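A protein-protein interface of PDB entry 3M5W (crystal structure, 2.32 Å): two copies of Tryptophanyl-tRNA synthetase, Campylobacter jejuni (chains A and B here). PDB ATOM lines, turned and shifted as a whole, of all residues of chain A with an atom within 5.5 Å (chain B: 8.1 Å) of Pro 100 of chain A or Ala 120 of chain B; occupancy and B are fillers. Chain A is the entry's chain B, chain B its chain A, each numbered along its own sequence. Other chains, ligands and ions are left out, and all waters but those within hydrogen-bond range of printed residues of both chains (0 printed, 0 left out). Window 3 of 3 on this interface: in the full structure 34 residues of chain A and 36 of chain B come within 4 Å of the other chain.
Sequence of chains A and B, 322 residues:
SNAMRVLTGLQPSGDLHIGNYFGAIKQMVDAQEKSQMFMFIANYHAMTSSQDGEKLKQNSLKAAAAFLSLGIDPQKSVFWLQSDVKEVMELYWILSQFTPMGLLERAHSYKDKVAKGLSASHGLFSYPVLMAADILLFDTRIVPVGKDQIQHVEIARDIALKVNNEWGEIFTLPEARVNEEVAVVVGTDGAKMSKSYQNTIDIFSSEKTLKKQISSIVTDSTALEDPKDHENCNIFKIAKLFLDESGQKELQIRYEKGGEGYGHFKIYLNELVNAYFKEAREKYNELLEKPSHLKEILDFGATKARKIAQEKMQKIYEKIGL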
ATOM      1  N   PHE A  98     -31.666  -5.750  11.876  1.00  0.00           N
ATOM      2  CA  PHE A  98     -32.189  -6.080  13.193  1.00  0.00           C
ATOM      3  C   PHE A  98     -31.060  -6.588  14.098  1.00  0.00           C
ATOM      4  O   PHE A  98     -31.319  -7.076  15.175  1.00  0.00           O
ATOM      5  CB  PHE A  98     -33.250  -7.211  13.094  1.00  0.00           C
ATOM      6  CG  PHE A  98     -34.517  -6.803  12.402  1.00  0.00           C
ATOM      7  CD1 PHE A  98     -35.547  -6.162  13.112  1.00  0.00           C
ATOM      8  CD2 PHE A  98     -34.698  -7.047  11.048  1.00  0.00           C
ATOM      9  CE1 PHE A  98     -36.735  -5.759  12.474  1.00  0.00           C
ATOM     10  CE2 PHE A  98     -35.887  -6.659  10.411  1.00  0.00           C
ATOM     11  CZ  PHE A  98     -36.910  -5.999  11.133  1.00  0.00           C
ATOM     12  N   THR A  99     -29.816  -6.533  13.647  1.00  0.00           N
ATOM     13  CA  THR A  99     -28.727  -7.105  14.442  1.00  0.00           C
ATOM     14  C   THR A  99     -27.795  -6.087  15.075  1.00  0.00           C
ATOM     15  O   THR A  99     -27.060  -5.407  14.384  1.00  0.00           O
ATOM     16  CB  THR A  99     -27.869  -8.060  13.606  1.00  0.00           C
ATOM     17  OG1 THR A  99     -28.709  -9.106  13.135  1.00  0.00           O
ATOM     18  CG2 THR A  99     -26.747  -8.651  14.452  1.00  0.00           C
ATOM     19  N   PRO A 100     -27.827  -5.991  16.407  1.00  0.00           N
ATOM     20  CA  PRO A 100     -27.036  -4.971  17.114  1.00  0.00           C
ATOM     21  C   PRO A 100     -25.547  -5.290  17.084  1.00  0.00           C
ATOM     22  O   PRO A 100     -25.167  -6.429  17.225  1.00  0.00           O
ATOM     23  CB  PRO A 100     -27.576  -5.033  18.556  1.00  0.00           C
ATOM     24  CG  PRO A 100     -28.930  -5.790  18.457  1.00  0.00           C
ATOM     25  CD  PRO A 100     -28.757  -6.722  17.294  1.00  0.00           C
ATOM     26  N   MET A 101     -24.711  -4.278  16.936  1.00  0.00           N
ATOM     27  CA  MET A 101     -23.275  -4.493  16.795  1.00  0.00           C
ATOM     28  C   MET A 101     -22.600  -5.299  17.927  1.00  0.00           C
ATOM     29  O   MET A 101     -21.801  -6.223  17.676  1.00  0.00           O
ATOM     30  CB  MET A 101     -22.584  -3.153  16.588  1.00  0.00           C
ATOM     31  CG  MET A 101     -22.792  -2.586  15.172  1.00  0.00           C
ATOM     32  SD  MET A 101     -21.766  -3.618  13.848  1.00  0.00           S
ATOM     33  CE  MET A 101     -19.956  -3.151  14.496  1.00  0.00           C
ATOM     34  N   GLY A 102     -22.926  -4.952  19.159  1.00  0.00           N
ATOM     35  CA  GLY A 102     -22.408  -5.653  20.315  1.00  0.00           C
ATOM     36  C   GLY A 102     -22.679  -7.142  20.326  1.00  0.00           C
ATOM     37  O   GLY A 102     -21.912  -7.916  20.892  1.00  0.00           O
ATOM     38  N   LEU A 103     -23.764  -7.551  19.683  1.00  0.00           N
ATOM     39  CA  LEU A 103     -24.056  -8.965  19.534  1.00  0.00           C
ATOM     40  C   LEU A 103     -22.957  -9.681  18.700  1.00  0.00           C
ATOM     41  O   LEU A 103     -22.587 -10.844  19.003  1.00  0.00           O
ATOM     42  CB  LEU A 103     -25.450  -9.129  18.905  1.00  0.00           C
ATOM     43  CG  LEU A 103     -26.282 -10.372  19.226  1.00  0.00           C
ATOM     44  CD1 LEU A 103     -26.468 -10.523  20.743  1.00  0.00           C
ATOM     45  CD2 LEU A 103     -27.617 -10.326  18.513  1.00  0.00           C
ATOM     46  N   LEU A 104     -22.423  -8.989  17.680  1.00  0.00           N
ATOM     47  CA  LEU A 104     -21.308  -9.517  16.896  1.00  0.00           C
ATOM     48  C   LEU A 104     -19.920  -9.258  17.508  1.00  0.00           C
ATOM     49  O   LEU A 104     -19.038 -10.096  17.428  1.00  0.00           O
ATOM     50  CB  LEU A 104     -21.351  -9.015  15.444  1.00  0.00           C
ATOM     51  CG  LEU A 104     -22.723  -9.273  14.788  1.00  0.00           C
ATOM     52  CD1 LEU A 104     -22.796  -8.609  13.438  1.00  0.00           C
ATOM     53  CD2 LEU A 104     -23.067 -10.754  14.722  1.00  0.00           C
ATOM     54  N   LYS A 162     -35.987  -9.953  18.041  1.00  0.00           N
ATOM     55  CA  LYS A 162     -35.954  -8.617  17.490  1.00  0.00           C
ATOM     56  C   LYS A 162     -36.945  -8.464  16.359  1.00  0.00           C
ATOM     57  O   LYS A 162     -37.821  -7.610  16.405  1.00  0.00           O
ATOM     58  CB  LYS A 162     -34.539  -8.239  17.053  1.00  0.00           C
ATOM     59  CG  LYS A 162     -34.398  -6.739  16.726  1.00  0.00           C
ATOM     60  CD  LYS A 162     -33.726  -5.903  17.840  1.00  0.00           C
ATOM     61  CE  LYS A 162     -33.927  -4.372  17.664  1.00  0.00           C
ATOM     62  NZ  LYS A 162     -32.830  -3.671  16.906  1.00  0.00           N
ATOM     63  N   TYR B 110     -21.194   5.517   9.541  1.00  0.00           N
ATOM     64  CA  TYR B 110     -21.242   4.747  10.778  1.00  0.00           C
ATOM     65  C   TYR B 110     -20.510   5.468  11.905  1.00  0.00           C
ATOM     66  O   TYR B 110     -21.080   5.721  12.967  1.00  0.00           O
ATOM     67  CB  TYR B 110     -20.641   3.356  10.567  1.00  0.00           C
ATOM     68  CG  TYR B 110     -20.223   2.669  11.847  1.00  0.00           C
ATOM     69  CD1 TYR B 110     -21.169   2.152  12.723  1.00  0.00           C
ATOM     70  CD2 TYR B 110     -18.881   2.538  12.181  1.00  0.00           C
ATOM     71  CE1 TYR B 110     -20.792   1.523  13.894  1.00  0.00           C
ATOM     72  CE2 TYR B 110     -18.495   1.911  13.351  1.00  0.00           C
ATOM     73  CZ  TYR B 110     -19.453   1.405  14.203  1.00  0.00           C
ATOM     74  OH  TYR B 110     -19.072   0.780  15.368  1.00  0.00           O
ATOM     75  N   ALA B 120     -26.853   1.557  16.330  1.00  0.00           N
ATOM     76  CA  ALA B 120     -25.802   0.959  15.482  1.00  0.00           C
ATOM     77  C   ALA B 120     -26.009  -0.543  15.172  1.00  0.00           C
ATOM     78  O   ALA B 120     -25.645  -1.424  15.968  1.00  0.00           O
ATOM     79  CB  ALA B 120     -24.420   1.205  16.079  1.00  0.00           C
ATOM     80  N   SER B 121     -26.632  -0.800  14.024  1.00  0.00           N
ATOM     81  CA  SER B 121     -27.009  -2.134  13.582  1.00  0.00           C
ATOM     82  C   SER B 121     -25.964  -2.627  12.573  1.00  0.00           C
ATOM     83  O   SER B 121     -25.241  -1.824  11.984  1.00  0.00           O
ATOM     84  CB  SER B 121     -28.334  -2.050  12.861  1.00  0.00           C
ATOM     85  OG  SER B 121     -28.062  -1.542  11.574  1.00  0.00           O
ATOM     86  N   HIS B 122     -25.869  -3.936  12.367  1.00  0.00           N
ATOM     87  CA  HIS B 122     -24.886  -4.469  11.416  1.00  0.00           C
ATOM     88  C   HIS B 122     -25.193  -3.974   9.980  1.00  0.00           C
ATOM     89  O   HIS B 122     -24.290  -3.705   9.209  1.00  0.00           O
ATOM     90  CB  HIS B 122     -24.853  -6.000  11.550  1.00  0.00           C
ATOM     91  CG  HIS B 122     -23.909  -6.698  10.609  1.00  0.00           C
ATOM     92  ND1 HIS B 122     -24.326  -7.271   9.424  1.00  0.00           N
ATOM     93  CD2 HIS B 122     -22.587  -6.972  10.710  1.00  0.00           C
ATOM     94  CE1 HIS B 122     -23.305  -7.861   8.832  1.00  0.00           C
ATOM     95  NE2 HIS B 122     -22.237  -7.693   9.593  1.00  0.00           N
ATOM     96  N   GLY B 123     -26.473  -3.803   9.640  1.00  0.00           N
ATOM     97  CA  GLY B 123     -26.889  -3.197   8.360  1.00  0.00           C
ATOM     98  C   GLY B 123     -26.157  -1.902   8.074  1.00  0.00           C
ATOM     99  O   GLY B 123     -25.688  -1.634   6.945  1.00  0.00           O
ATOM    100  N   LEU B 124     -26.042  -1.087   9.124  1.00  0.00           N
ATOM    101  CA  LEU B 124     -25.510   0.265   9.002  1.00  0.00           C
ATOM    102  C   LEU B 124     -24.001   0.236   8.893  1.00  0.00           C
ATOM    103  O   LEU B 124     -23.387   0.947   8.104  1.00  0.00           O
ATOM    104  CB  LEU B 124     -25.922   1.135  10.201  1.00  0.00           C
ATOM    105  CG  LEU B 124     -25.444   2.548   9.940  1.00  0.00           C
ATOM    106  CD1 LEU B 124     -26.264   3.053   8.747  1.00  0.00           C
ATOM    107  CD2 LEU B 124     -25.583   3.430  11.147  1.00  0.00           C
ATOM    108  N   PHE B 125     -23.401  -0.597   9.715  1.00  0.00           N
ATOM    109  CA  PHE B 125     -21.969  -0.806   9.625  1.00  0.00           C
ATOM    110  C   PHE B 125     -21.540  -1.343   8.253  1.00  0.00           C
ATOM    111  O   PHE B 125     -20.497  -0.973   7.729  1.00  0.00           O
ATOM    112  CB  PHE B 125     -21.556  -1.738  10.751  1.00  0.00           C
ATOM    113  CG  PHE B 125     -20.084  -1.983  10.824  1.00  0.00           C
ATOM    114  CD1 PHE B 125     -19.225  -0.974  11.215  1.00  0.00           C
ATOM    115  CD2 PHE B 125     -19.560  -3.243  10.533  1.00  0.00           C
ATOM    116  CE1 PHE B 125     -17.862  -1.182  11.278  1.00  0.00           C
ATOM    117  CE2 PHE B 125     -18.172  -3.477  10.609  1.00  0.00           C
ATOM    118  CZ  PHE B 125     -17.319  -2.449  10.977  1.00  0.00           C
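Of the 7 printed residues of chain B, 4 touch a printed residue of chain A.
Hydrophobic or aromatic side chains of chain B within 4 Å of the printed part of chain A: His 122 and Phe 125.
Printed residues of chain A that touch a printed residue of chain B: Thr 99, Pro 100, Met 101 and Leu 104.
Among the printed residues, 6 pairs touch across the chains.
Among the printed residues, no Asp or Glu carboxylate lies within 4 Å of a Lys or Arg side-chain nitrogen of the other chain.
Ser 121 of chain B touches Thr 99 of chain A.
O of Ala 120 of chain B touches CA of Pro 100 of chain A (3.98 Å).
Met 101 of chain A touches Phe 125 of chain B.
Leu 104 of chain A touches His 122 of chain B.
Printed residues of chain B within 4 Å of Thr 99 of chain A: Ser 121 (3.4 Å) and His 122 (2.8 Å).
Pro 100 of chain A touches one residue of chain B.
Of the printed residues of chain B, Met 101 of chain A touches Ala 120 and Phe 125.
Printed residues of chain A within 4 Å of His 122 of chain B: Thr 99 and Leu 104.
The nearest printed residue of chain B that does not touch Leu 104 of chain A is Ser 121 of chain B (6.8 Å).
No position is printed for both chains.
Of the 6 pairs that touch across the chains among the printed residues, none has its exchanged pair printed and touching as well.
The backbone NH (N) of Gly 123 of chain B lies close to the side-chain hydroxyl (OG) of Ser 121 of chain B (3.4 Å).
The backbone NH (N) of Leu 124 of chain B sits at hydrogen-bond distance from the side-chain hydroxyl (OG) of Ser 121 of chain B, at 3.2 Å.
The backbone NH (N) of Met 101 of chain A lies within hydrogen-bond range of the backbone carbonyl oxygen (O) of Ala 120 of chain B (3.2 Å).
The backbone NH of His 122 of chain B lies within hydrogen-bond range of the backbone carbonyl oxygen of Thr 99 of chain A.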
